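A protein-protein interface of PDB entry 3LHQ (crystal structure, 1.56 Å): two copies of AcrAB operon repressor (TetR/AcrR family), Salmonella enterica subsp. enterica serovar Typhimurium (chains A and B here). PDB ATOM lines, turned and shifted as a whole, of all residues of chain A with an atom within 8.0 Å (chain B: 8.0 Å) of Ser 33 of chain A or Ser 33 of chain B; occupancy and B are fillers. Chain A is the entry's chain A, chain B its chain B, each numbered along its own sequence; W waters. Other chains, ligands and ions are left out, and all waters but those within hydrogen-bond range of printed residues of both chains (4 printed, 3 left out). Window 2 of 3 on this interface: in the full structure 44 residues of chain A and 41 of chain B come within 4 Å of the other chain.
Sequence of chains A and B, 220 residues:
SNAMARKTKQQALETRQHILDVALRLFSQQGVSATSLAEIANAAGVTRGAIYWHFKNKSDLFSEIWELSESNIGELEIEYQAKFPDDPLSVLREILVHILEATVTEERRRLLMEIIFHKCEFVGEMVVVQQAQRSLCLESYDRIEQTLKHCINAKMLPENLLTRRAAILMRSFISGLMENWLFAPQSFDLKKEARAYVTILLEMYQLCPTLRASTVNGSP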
ATOM      1  N   PHE A  27     -21.682 -18.485   6.929  1.00  0.00           N
ATOM      2  CA  PHE A  27     -22.577 -19.008   7.953  1.00  0.00           C
ATOM      3  C   PHE A  27     -22.052 -20.273   8.618  1.00  0.00           C
ATOM      4  O   PHE A  27     -22.164 -20.432   9.839  1.00  0.00           O
ATOM      5  CB  PHE A  27     -23.959 -19.342   7.371  1.00  0.00           C
ATOM      6  CG  PHE A  27     -24.819 -18.180   6.927  1.00  0.00           C
ATOM      7  CD1 PHE A  27     -24.689 -16.900   7.468  1.00  0.00           C
ATOM      8  CD2 PHE A  27     -25.841 -18.413   6.038  1.00  0.00           C
ATOM      9  CE1 PHE A  27     -25.561 -15.862   7.104  1.00  0.00           C
ATOM     10  CE2 PHE A  27     -26.710 -17.403   5.652  1.00  0.00           C
ATOM     11  CZ  PHE A  27     -26.574 -16.107   6.208  1.00  0.00           C
ATOM     12  N   GLN A  30     -18.915 -18.994  10.937  1.00  0.00           N
ATOM     13  CA  GLN A  30     -19.107 -18.073  12.090  1.00  0.00           C
ATOM     14  C   GLN A  30     -20.511 -18.006  12.632  1.00  0.00           C
ATOM     15  O   GLN A  30     -20.717 -17.317  13.631  1.00  0.00           O
ATOM     16  CB  GLN A  30     -18.555 -16.687  11.818  1.00  0.00           C
ATOM     17  CG  GLN A  30     -19.028 -16.125  10.565  1.00  0.00           C
ATOM     18  CD  GLN A  30     -18.493 -14.748  10.309  1.00  0.00           C
ATOM     19  OE1 GLN A  30     -17.323 -14.509  10.481  1.00  0.00           O
ATOM     20  NE2 GLN A  30     -19.349 -13.844   9.861  1.00  0.00           N
ATOM     21  N   GLY A  31     -21.448 -18.767  12.062  1.00  0.00           N
ATOM     22  CA  GLY A  31     -22.833 -18.761  12.536  1.00  0.00           C
ATOM     23  C   GLY A  31     -23.647 -17.680  11.848  1.00  0.00           C
ATOM     24  O   GLY A  31     -23.078 -16.673  11.378  1.00  0.00           O
ATOM     25  N   VAL A  32     -24.957 -17.893  11.750  1.00  0.00           N
ATOM     26  CA  VAL A  32     -25.862 -16.952  11.144  1.00  0.00           C
ATOM     27  C   VAL A  32     -25.956 -15.640  11.979  1.00  0.00           C
ATOM     28  O   VAL A  32     -25.879 -14.543  11.423  1.00  0.00           O
ATOM     29  CB  VAL A  32     -27.261 -17.630  10.839  1.00  0.00           C
ATOM     30  CG1 VAL A  32     -28.292 -16.595  10.372  1.00  0.00           C
ATOM     31  CG2 VAL A  32     -27.143 -18.701   9.853  1.00  0.00           C
ATOM     32  N   SER A  33     -25.992 -15.729  13.306  1.00  0.00           N
ATOM     33  CA  SER A  33     -26.223 -14.561  14.139  1.00  0.00           C
ATOM     34  C   SER A  33     -25.120 -13.483  13.949  1.00  0.00           C
ATOM     35  O   SER A  33     -25.388 -12.291  13.856  1.00  0.00           O
ATOM     36  CB  SER A  33     -26.307 -14.969  15.621  1.00  0.00           C
ATOM     37  OG  SER A  33     -27.550 -15.632  15.883  1.00  0.00           O
ATOM     38  N   ALA A  34     -23.874 -13.912  13.930  1.00  0.00           N
ATOM     39  CA  ALA A  34     -22.721 -13.015  13.750  1.00  0.00           C
ATOM     40  C   ALA A  34     -22.456 -12.516  12.326  1.00  0.00           C
ATOM     41  O   ALA A  34     -21.577 -11.681  12.101  1.00  0.00           O
ATOM     42  CB  ALA A  34     -21.468 -13.676  14.272  1.00  0.00           C
ATOM     43  N   THR A  35     -23.171 -13.068  11.365  1.00  0.00           N
ATOM     44  CA  THR A  35     -22.901 -12.768   9.954  1.00  0.00           C
ATOM     45  C   THR A  35     -23.902 -11.791   9.415  1.00  0.00           C
ATOM     46  O   THR A  35     -25.088 -12.032   9.471  1.00  0.00           O
ATOM     47  CB  THR A  35     -22.968 -14.062   9.069  1.00  0.00           C
ATOM     48  OG1 THR A  35     -22.013 -15.008   9.523  1.00  0.00           O
ATOM     49  CG2 THR A  35     -22.727 -13.738   7.587  1.00  0.00           C
ATOM     50  N   SER A  36     -23.437 -10.651   8.922  1.00  0.00           N
ATOM     51  CA  SER A  36     -24.338  -9.696   8.263  1.00  0.00           C
ATOM     52  C   SER A  36     -24.343  -9.788   6.724  1.00  0.00           C
ATOM     53  O   SER A  36     -23.403 -10.302   6.099  1.00  0.00           O
ATOM     54  CB  SER A  36     -23.881  -8.248   8.596  1.00  0.00           C
ATOM     55  OG  SER A  36     -22.535  -8.029   8.103  1.00  0.00           O
ATOM     56  N   GLU A  39     -21.223  -8.189   5.383  1.00  0.00           N
ATOM     57  CA  GLU A  39     -20.110  -9.102   5.412  1.00  0.00           C
ATOM     58  C   GLU A  39     -20.123 -10.064   4.227  1.00  0.00           C
ATOM     59  O   GLU A  39     -19.113 -10.318   3.567  1.00  0.00           O
ATOM     60  CB  GLU A  39     -20.157  -9.905   6.722  1.00  0.00           C
ATOM     61  CG  GLU A  39     -19.472  -9.258   7.916  1.00  0.00           C
ATOM     62  CD  GLU A  39     -19.510 -10.193   9.076  1.00  0.00           C
ATOM     63  OE1 GLU A  39     -18.523 -10.940   9.235  1.00  0.00           O
ATOM     64  OE2 GLU A  39     -20.546 -10.238   9.744  1.00  0.00           O
ATOM     65  N   LYS A  58     -31.046 -11.602   5.842  1.00  0.00           N
ATOM     66  CA  LYS A  58     -30.269 -12.822   5.799  1.00  0.00           C
ATOM     67  C   LYS A  58     -31.119 -14.059   5.963  1.00  0.00           C
ATOM     68  O   LYS A  58     -30.778 -15.117   5.407  1.00  0.00           O
ATOM     69  CB  LYS A  58     -29.075 -12.757   6.752  1.00  0.00           C
ATOM     70  CG  LYS A  58     -29.356 -12.863   8.145  1.00  0.00           C
ATOM     71  CD  LYS A  58     -28.094 -12.741   8.985  1.00  0.00           C
ATOM     72  CE  LYS A  58     -28.455 -12.438  10.427  1.00  0.00           C
ATOM     73  NZ  LYS A  58     -27.203 -12.080  11.185  1.00  0.00           N
ATOM     74  N   LYS A 119     -25.483 -24.207  13.180  1.00  0.00           N
ATOM     75  CA  LYS A 119     -24.960 -22.856  12.999  1.00  0.00           C
ATOM     76  C   LYS A 119     -26.019 -21.787  12.865  1.00  0.00           C
ATOM     77  O   LYS A 119     -25.727 -20.702  12.356  1.00  0.00           O
ATOM     78  CB  LYS A 119     -23.995 -22.759  11.836  1.00  0.00           C
ATOM     79  CG  LYS A 119     -22.840 -23.756  11.983  1.00  0.00           C
ATOM     80  CD  LYS A 119     -21.811 -23.304  12.984  1.00  0.00           C
ATOM     81  CE  LYS A 119     -20.772 -24.383  13.329  1.00  0.00           C
ATOM     82  NZ  LYS A 119     -19.989 -24.900  12.162  1.00  0.00           N
ATOM     83  N   CYS A 120     -27.274 -22.081  13.280  1.00  0.00           N
ATOM     84  CA  CYS A 120     -28.458 -21.149  13.112  1.00  0.00           C
ATOM     85  C   CYS A 120     -29.492 -21.251  14.258  1.00  0.00           C
ATOM     86  O   CYS A 120     -30.180 -22.255  14.357  1.00  0.00           O
ATOM     87  CB  CYS A 120     -29.232 -21.428  11.817  1.00  0.00           C
ATOM     88  SG  CYS A 120     -30.621 -20.245  11.384  1.00  0.00           S
ATOM     89  N   GLU A 121     -29.698 -20.176  15.027  1.00  0.00           N
ATOM     90  CA  GLU A 121     -30.684 -20.187  16.085  1.00  0.00           C
ATOM     91  C   GLU A 121     -32.018 -19.770  15.439  1.00  0.00           C
ATOM     92  O   GLU A 121     -32.071 -18.819  14.683  1.00  0.00           O
ATOM     93  CB  GLU A 121     -30.295 -19.210  17.166  1.00  0.00           C
ATOM     94  CG  GLU A 121     -28.989 -19.549  17.866  1.00  0.00           C
ATOM     95  CD  GLU A 121     -28.508 -18.534  18.910  1.00  0.00           C
ATOM     96  OE1 GLU A 121     -29.138 -17.508  19.080  1.00  0.00           O
ATOM     97  OE2 GLU A 121     -27.479 -18.796  19.551  1.00  0.00           O
ATOM     98  N   PHE A 122     -33.057 -20.548  15.690  1.00  0.00           N
ATOM     99  CA  PHE A 122     -34.337 -20.312  15.113  1.00  0.00           C
ATOM    100  C   PHE A 122     -35.094 -19.289  15.992  1.00  0.00           C
ATOM    101  O   PHE A 122     -36.048 -19.597  16.707  1.00  0.00           O
ATOM    102  CB  PHE A 122     -35.052 -21.624  14.930  1.00  0.00           C
ATOM    103  CG  PHE A 122     -34.469 -22.423  13.855  1.00  0.00           C
ATOM    104  CD1 PHE A 122     -34.659 -22.076  12.521  1.00  0.00           C
ATOM    105  CD2 PHE A 122     -33.662 -23.486  14.145  1.00  0.00           C
ATOM    106  CE1 PHE A 122     -34.053 -22.826  11.491  1.00  0.00           C
ATOM    107  CE2 PHE A 122     -33.090 -24.212  13.179  1.00  0.00           C
ATOM    108  CZ  PHE A 122     -33.287 -23.880  11.817  1.00  0.00           C
ATOM    109  N   VAL A 123     -34.608 -18.061  15.951  1.00  0.00           N
ATOM    110  CA  VAL A 123     -35.131 -16.921  16.741  1.00  0.00           C
ATOM    111  C   VAL A 123     -35.108 -15.652  15.859  1.00  0.00           C
ATOM    112  O   VAL A 123     -34.411 -15.611  14.839  1.00  0.00           O
ATOM    113  CB  VAL A 123     -34.288 -16.628  18.009  1.00  0.00           C
ATOM    114  CG1 VAL A 123     -34.310 -17.805  18.930  1.00  0.00           C
ATOM    115  CG2 VAL A 123     -32.847 -16.325  17.647  1.00  0.00           C
ATOM    116  N   MET A 126     -35.361 -15.583  11.970  1.00  0.00           N
ATOM    117  CA  MET A 126     -35.301 -17.011  11.656  1.00  0.00           C
ATOM    118  C   MET A 126     -36.518 -17.793  12.082  1.00  0.00           C
ATOM    119  O   MET A 126     -36.722 -18.951  11.663  1.00  0.00           O
ATOM    120  CB  MET A 126     -34.070 -17.704  12.283  1.00  0.00           C
ATOM    121  CG  MET A 126     -32.790 -17.472  11.582  1.00  0.00           C
ATOM    122  SD  MET A 126     -32.826 -17.772   9.807  1.00  0.00           S
ATOM    123  CE  MET A 126     -32.043 -16.226   9.530  1.00  0.00           C
ATOM    124  N   PHE B  27     -32.702 -18.924  27.128  1.00  0.00           N
ATOM    125  CA  PHE B  27     -32.024 -19.414  25.937  1.00  0.00           C
ATOM    126  C   PHE B  27     -33.017 -20.047  24.990  1.00  0.00           C
ATOM    127  O   PHE B  27     -32.933 -19.917  23.745  1.00  0.00           O
ATOM    128  CB  PHE B  27     -31.013 -20.478  26.283  1.00  0.00           C
ATOM    129  CG  PHE B  27     -29.764 -20.001  26.972  1.00  0.00           C
ATOM    130  CD1 PHE B  27     -29.305 -18.711  26.809  1.00  0.00           C
ATOM    131  CD2 PHE B  27     -28.996 -20.906  27.690  1.00  0.00           C
ATOM    132  CE1 PHE B  27     -28.131 -18.309  27.394  1.00  0.00           C
ATOM    133  CE2 PHE B  27     -27.844 -20.519  28.314  1.00  0.00           C
ATOM    134  CZ  PHE B  27     -27.387 -19.208  28.144  1.00  0.00           C
ATOM    135  N   GLN B  30     -35.080 -16.935  23.370  1.00  0.00           N
ATOM    136  CA  GLN B  30     -34.308 -15.865  22.730  1.00  0.00           C
ATOM    137  C   GLN B  30     -33.082 -16.339  21.980  1.00  0.00           C
ATOM    138  O   GLN B  30     -32.490 -15.583  21.178  1.00  0.00           O
ATOM    139  CB  GLN B  30     -33.733 -14.910  23.792  1.00  0.00           C
ATOM    140  CG  GLN B  30     -34.617 -14.174  24.643  1.00  0.00           C
ATOM    141  CD  GLN B  30     -33.898 -12.911  25.088  1.00  0.00           C
ATOM    142  OE1 GLN B  30     -34.327 -11.809  24.763  1.00  0.00           O
ATOM    143  NE2 GLN B  30     -32.760 -13.066  25.765  1.00  0.00           N
ATOM    144  N   GLY B  31     -32.643 -17.557  22.264  1.00  0.00           N
ATOM    145  CA  GLY B  31     -31.366 -18.053  21.712  1.00  0.00           C
ATOM    146  C   GLY B  31     -30.180 -17.737  22.580  1.00  0.00           C
ATOM    147  O   GLY B  31     -30.190 -16.746  23.337  1.00  0.00           O
ATOM    148  N   VAL B  32     -29.129 -18.536  22.493  1.00  0.00           N
ATOM    149  CA  VAL B  32     -27.928 -18.303  23.287  1.00  0.00           C
ATOM    150  C   VAL B  32     -27.222 -17.018  22.849  1.00  0.00           C
ATOM    151  O   VAL B  32     -26.858 -16.207  23.695  1.00  0.00           O
ATOM    152  CB  VAL B  32     -26.993 -19.560  23.269  1.00  0.00           C
ATOM    153  CG1 VAL B  32     -25.668 -19.256  23.925  1.00  0.00           C
ATOM    154  CG2 VAL B  32     -27.711 -20.769  23.920  1.00  0.00           C
ATOM    155  N   SER B  33     -27.136 -16.746  21.557  1.00  0.00           N
ATOM    156  CA  SER B  33     -26.303 -15.644  21.087  1.00  0.00           C
ATOM    157  C   SER B  33     -26.834 -14.271  21.597  1.00  0.00           C
ATOM    158  O   SER B  33     -26.016 -13.397  21.964  1.00  0.00           O
ATOM    159  CB  SER B  33     -26.141 -15.685  19.543  1.00  0.00           C
ATOM    160  OG  SER B  33     -25.437 -16.884  19.103  1.00  0.00           O
ATOM    161  N   ALA B  34     -28.161 -14.089  21.616  1.00  0.00           N
ATOM    162  CA  ALA B  34     -28.836 -12.856  22.076  1.00  0.00           C
ATOM    163  C   ALA B  34     -28.900 -12.652  23.563  1.00  0.00           C
ATOM    164  O   ALA B  34     -29.238 -11.559  24.023  1.00  0.00           O
ATOM    165  CB  ALA B  34     -30.268 -12.799  21.593  1.00  0.00           C
ATOM    166  N   THR B  35     -28.676 -13.713  24.311  1.00  0.00           N
ATOM    167  CA  THR B  35     -28.959 -13.692  25.735  1.00  0.00           C
ATOM    168  C   THR B  35     -27.698 -13.448  26.481  1.00  0.00           C
ATOM    169  O   THR B  35     -26.757 -14.233  26.399  1.00  0.00           O
ATOM    170  CB  THR B  35     -29.556 -15.042  26.200  1.00  0.00           C
ATOM    171  OG1 THR B  35     -30.819 -15.240  25.561  1.00  0.00           O
ATOM    172  CG2 THR B  35     -29.753 -15.040  27.727  1.00  0.00           C
ATOM    173  N   SER B  36     -27.638 -12.357  27.228  1.00  0.00           N
ATOM    174  CA  SER B  36     -26.452 -12.136  28.045  1.00  0.00           C
ATOM    175  C   SER B  36     -26.592 -12.680  29.467  1.00  0.00           C
ATOM    176  O   SER B  36     -27.721 -12.854  29.990  1.00  0.00           O
ATOM    177  CB  SER B  36     -26.178 -10.639  28.190  1.00  0.00           C
ATOM    178  OG  SER B  36     -27.210 -10.005  28.913  1.00  0.00           O
ATOM    179  N   GLU B  39     -28.709 -10.354  31.437  1.00  0.00           N
ATOM    180  CA  GLU B  39     -30.130 -10.569  31.240  1.00  0.00           C
ATOM    181  C   GLU B  39     -30.577 -11.725  32.141  1.00  0.00           C
ATOM    182  O   GLU B  39     -31.633 -11.685  32.779  1.00  0.00           O
ATOM    183  CB  GLU B  39     -30.411 -10.913  29.749  1.00  0.00           C
ATOM    184  CG  GLU B  39     -30.426  -9.722  28.810  1.00  0.00           C
ATOM    185  CD  GLU B  39     -30.860 -10.102  27.425  1.00  0.00           C
ATOM    186  OE1 GLU B  39     -32.084 -10.090  27.166  1.00  0.00           O
ATOM    187  OE2 GLU B  39     -29.987 -10.414  26.604  1.00  0.00           O
ATOM    188  N   LYS B  58     -21.484 -17.706  29.109  1.00  0.00           N
ATOM    189  CA  LYS B  58     -22.713 -18.431  28.793  1.00  0.00           C
ATOM    190  C   LYS B  58     -22.430 -19.881  28.530  1.00  0.00           C
ATOM    191  O   LYS B  58     -23.298 -20.724  28.818  1.00  0.00           O
ATOM    192  CB  LYS B  58     -23.358 -17.961  27.483  1.00  0.00           C
ATOM    193  CG  LYS B  58     -23.735 -16.610  27.312  1.00  0.00           C
ATOM    194  CD  LYS B  58     -23.884 -16.364  25.763  1.00  0.00           C
ATOM    195  CE  LYS B  58     -23.963 -14.934  25.423  1.00  0.00           C
ATOM    196  NZ  LYS B  58     -25.042 -14.492  24.487  1.00  0.00           N
ATOM    197  N   LYS B 119     -31.369 -23.684  19.273  1.00  0.00           N
ATOM    198  CA  LYS B 119     -31.220 -22.370  19.854  1.00  0.00           C
ATOM    199  C   LYS B 119     -29.820 -22.000  20.282  1.00  0.00           C
ATOM    200  O   LYS B 119     -29.639 -21.043  21.061  1.00  0.00           O
ATOM    201  CB  LYS B 119     -32.232 -22.156  21.025  1.00  0.00           C
ATOM    202  CG  LYS B 119     -33.694 -22.468  20.663  1.00  0.00           C
ATOM    203  CD  LYS B 119     -34.289 -21.304  19.959  1.00  0.00           C
ATOM    204  CE  LYS B 119     -35.690 -21.607  19.408  1.00  0.00           C
ATOM    205  NZ  LYS B 119     -36.768 -21.964  20.395  1.00  0.00           N
ATOM    206  N   CYS B 120     -28.803 -22.709  19.757  1.00  0.00           N
ATOM    207  CA  CYS B 120     -27.377 -22.472  20.072  1.00  0.00           C
ATOM    208  C   CYS B 120     -26.423 -22.751  18.890  1.00  0.00           C
ATOM    209  O   CYS B 120     -26.266 -23.906  18.420  1.00  0.00           O
ATOM    210  CB  CYS B 120     -26.938 -23.305  21.283  1.00  0.00           C
ATOM    211  SG  CYS B 120     -25.189 -23.156  21.834  1.00  0.00           S
ATOM    212  N   GLU B 121     -25.728 -21.708  18.454  1.00  0.00           N
ATOM    213  CA  GLU B 121     -24.794 -21.848  17.367  1.00  0.00           C
ATOM    214  C   GLU B 121     -23.481 -22.332  17.979  1.00  0.00           C
ATOM    215  O   GLU B 121     -23.042 -21.767  19.001  1.00  0.00           O
ATOM    216  CB  GLU B 121     -24.538 -20.523  16.660  1.00  0.00           C
ATOM    217  CG  GLU B 121     -25.753 -19.997  15.936  1.00  0.00           C
ATOM    218  CD  GLU B 121     -25.561 -18.656  15.320  1.00  0.00           C
ATOM    219  OE1 GLU B 121     -24.474 -18.100  15.482  1.00  0.00           O
ATOM    220  OE2 GLU B 121     -26.522 -18.186  14.703  1.00  0.00           O
ATOM    221  N   PHE B 122     -22.911 -23.383  17.384  1.00  0.00           N
ATOM    222  CA  PHE B 122     -21.657 -23.966  17.865  1.00  0.00           C
ATOM    223  C   PHE B 122     -20.445 -23.262  17.254  1.00  0.00           C
ATOM    224  O   PHE B 122     -19.720 -23.809  16.443  1.00  0.00           O
ATOM    225  CB  PHE B 122     -21.632 -25.463  17.702  1.00  0.00           C
ATOM    226  CG  PHE B 122     -22.601 -26.162  18.589  1.00  0.00           C
ATOM    227  CD1 PHE B 122     -22.282 -26.427  19.926  1.00  0.00           C
ATOM    228  CD2 PHE B 122     -23.860 -26.502  18.131  1.00  0.00           C
ATOM    229  CE1 PHE B 122     -23.193 -27.087  20.753  1.00  0.00           C
ATOM    230  CE2 PHE B 122     -24.756 -27.117  18.941  1.00  0.00           C
ATOM    231  CZ  PHE B 122     -24.422 -27.431  20.236  1.00  0.00           C
ATOM    232  N   VAL B 123     -20.246 -22.044  17.761  1.00  0.00           N
ATOM    233  CA  VAL B 123     -19.227 -21.148  17.360  1.00  0.00           C
ATOM    234  C   VAL B 123     -18.706 -20.375  18.560  1.00  0.00           C
ATOM    235  O   VAL B 123     -19.360 -20.345  19.595  1.00  0.00           O
ATOM    236  CB  VAL B 123     -19.748 -20.094  16.331  1.00  0.00           C
ATOM    237  CG1 VAL B 123     -20.282 -20.759  15.042  1.00  0.00           C
ATOM    238  CG2 VAL B 123     -20.748 -19.108  16.971  1.00  0.00           C
ATOM    239  N   GLU B 125     -17.065 -19.426  21.875  1.00  0.00           N
ATOM    240  CA  GLU B 125     -16.890 -20.136  23.116  1.00  0.00           C
ATOM    241  C   GLU B 125     -17.640 -21.496  23.089  1.00  0.00           C
ATOM    242  O   GLU B 125     -17.211 -22.487  23.743  1.00  0.00           O
ATOM    243  CB  GLU B 125     -17.312 -19.208  24.269  1.00  0.00           C
ATOM    244  CG  GLU B 125     -18.822 -19.130  24.493  1.00  0.00           C
ATOM    245  CD  GLU B 125     -19.316 -18.051  25.446  1.00  0.00           C
ATOM    246  OE1 GLU B 125     -20.113 -17.234  24.978  1.00  0.00           O
ATOM    247  OE2 GLU B 125     -18.951 -18.015  26.639  1.00  0.00           O
ATOM    248  N   MET B 126     -18.736 -21.587  22.311  1.00  0.00           N
ATOM    249  CA  MET B 126     -19.469 -22.842  22.190  1.00  0.00           C
ATOM    250  C   MET B 126     -18.686 -23.955  21.519  1.00  0.00           C
ATOM    251  O   MET B 126     -19.067 -25.133  21.575  1.00  0.00           O
ATOM    252  CB  MET B 126     -20.777 -22.631  21.423  1.00  0.00           C
ATOM    253  CG  MET B 126     -21.807 -21.820  22.156  1.00  0.00           C
ATOM    254  SD  MET B 126     -22.314 -22.700  23.620  1.00  0.00           S
ATOM    255  CE  MET B 126     -22.257 -21.306  24.691  1.00  0.00           C
HETATM  256  O   HOH W   1     -24.891 -19.399  20.324  1.00  0.00           O
HETATM  257  O   HOH W   2     -29.992 -15.351  20.062  1.00  0.00           O
HETATM  258  O   HOH W   3     -27.164 -24.241  15.813  1.00  0.00           O
HETATM  259  O   HOH W   4     -29.052 -17.454  14.013  1.00  0.00           O
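N of Val 32 of chain A is in hydrogen-bond range of OE2 of Glu 121 of chain B (3.4 Å).
OE2 of Glu 121 of chain B sits at hydrogen-bond distance from N of Ser 33 of chain A (2.9 Å).
OE2 of Glu 121 of chain A is in hydrogen-bond range of N of Val 32 of chain B, 3.4 Å away.
The side-chain hydroxyl (OG) of Ser 33 of chain B lies within hydrogen-bond range of the side-chain carboxylate (OE2) of Glu 121 of chain A.
The side-chain carboxylate (OE2) of Glu 121 of chain A sits close to the backbone carbonyl oxygen (O) of Lys 119 of chain B (3.5 Å).
O of Gly 31 of chain A sits at hydrogen-bond distance from OG1 of Thr 35 of chain A.
The side-chain amino group of Lys 58 of chain A lies within hydrogen-bond range of the backbone carbonyl oxygen of Val 32 of chain A (2.8 Å).
The backbone NH of Val 32 of chain A lies within hydrogen-bond range of the backbone carbonyl oxygen of Lys 119 of chain A.
The side-chain amide nitrogen (NE2) of Gln 30 of chain B sits at hydrogen-bond distance from the side-chain hydroxyl (OG1) of Thr 35 of chain B.
The side-chain amino group (NZ) of Lys 58 of chain B sits at hydrogen-bond distance from the backbone carbonyl oxygen (O) of Val 32 of chain B (2.6 Å).
The backbone carbonyl oxygen (O) of Lys 119 of chain B lies within hydrogen-bond range of the backbone NH (N) of Val 32 of chain B.
C of Gln 30 of chain A touches CG1 of Val 123 of chain B (3.7 Å).
Gly 31 of chain A touches Glu 121 of chain B.
Gly 31 of chain A touches Val 123 of chain B (N to CG1, 3.8 Å).
Ser 33 of chain A touches Ser 33 of chain B (OG to CB, 3.9 Å).
Lys 119 of chain A touches Glu 121 of chain B (O to OE2, 3.5 Å).
Lys 119 of chain A touches Phe 122 of chain B.
Lys 119 of chain A touches Val 123 of chain B.
Cys 120 of chain A touches Glu 121 of chain B.
Glu 121 of chain A touches Gly 31 of chain B.
Glu 121 of chain A touches Glu 121 of chain B (OE2 to N, 3.6 Å).
Printed residues of chain B within 4 Å of Gly 31 of chain A: Glu 121 and Val 123.
Of chain B, only Ser 33 and Glu 121 come within 4 Å of Ser 33 of chain A.
Ala 34 of chain A touches none of the printed residues of chain B.
Of the printed residues of chain B, Glu 121 of chain A touches Gly 31 (3.5 Å), Val 32 (3.4 Å), Ser 33 (2.8 Å), Lys 119 (3.5 Å), Cys 120 (3.7 Å) and Glu 121 (3.6 Å).
Printed residues of chain A within 4 Å of Gln 30 of chain B: Val 123 (3.6 Å).
The nearest residue of chain B that does not touch Ser 33 of chain A is Ala 34 of chain B (6.0 Å).
The nearest residue of chain A that does not touch Ser 33 of chain B is Ala 34 of chain A (6.2 Å).
The nearest printed residue of chain B that does not touch Val 123 of chain A is Phe 27 of chain B (5.4 Å).
Of the 16 printed residues of chain A, 9 touch a printed residue of chain B.
Hydrophobic or aromatic side chains of chain A within 4 Å of the printed part of chain B: Val 32 and Val 123.
Along chain A the printed residues that touch a printed residue of chain B span positions 30 to 123.
Of the 17 printed residues of chain B, 9 touch a printed residue of chain A.
Hydrophobic or aromatic side chains of chain B within 4 Å of the printed part of chain A: Val 32 and Val 123.
Among the printed residues, 20 pairs touch across the chains.
Lys 119 of chain A touches Glu 121 of chain B, and with the chains exchanged Glu 121 of chain A touches Lys 119 of chain B.
Lys 119 of chain A touches Phe 122 of chain B, and with the chains exchanged Phe 122 of chain A touches Lys 119 of chain B.
Cys 120 of chain A touches Glu 121 of chain B, and with the chains exchanged Glu 121 of chain A touches Cys 120 of chain B.
Glu 121 of chain B touches its own counterpart, Glu 121 of chain A.
Of the 20 pairs that touch across the chains among the printed residues, 20 have their exchanged pair printed and touching as well.
Water W2 lies within hydrogen-bond range of the side-chain carboxylate (OE1) of Glu 121 of chain A, the backbone NH (N) of Ala 34 of chain B and the backbone carbonyl oxygen (O) of Gln 30 of chain B.
Water W4 lies within hydrogen-bond range of OE2 of Glu 121 of chain B (2.7 Å), N of Glu 121 of chain A (3.0 Å) and OG of Ser 33 of chain A (3.0 Å).
Water W1 lies within hydrogen-bond range of the side-chain carboxylate of Glu 121 of chain A (2.8 Å), the side-chain hydroxyl of Ser 33 of chain B (2.8 Å) and the backbone NH of Glu 121 of chain B (3.1 Å).
Water W3 lies within hydrogen-bond range of O of Cys 120 of chain B (2.8 Å), N of Lys 119 of chain A (3.1 Å) and N of Cys 120 of chain A (3.3 Å).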
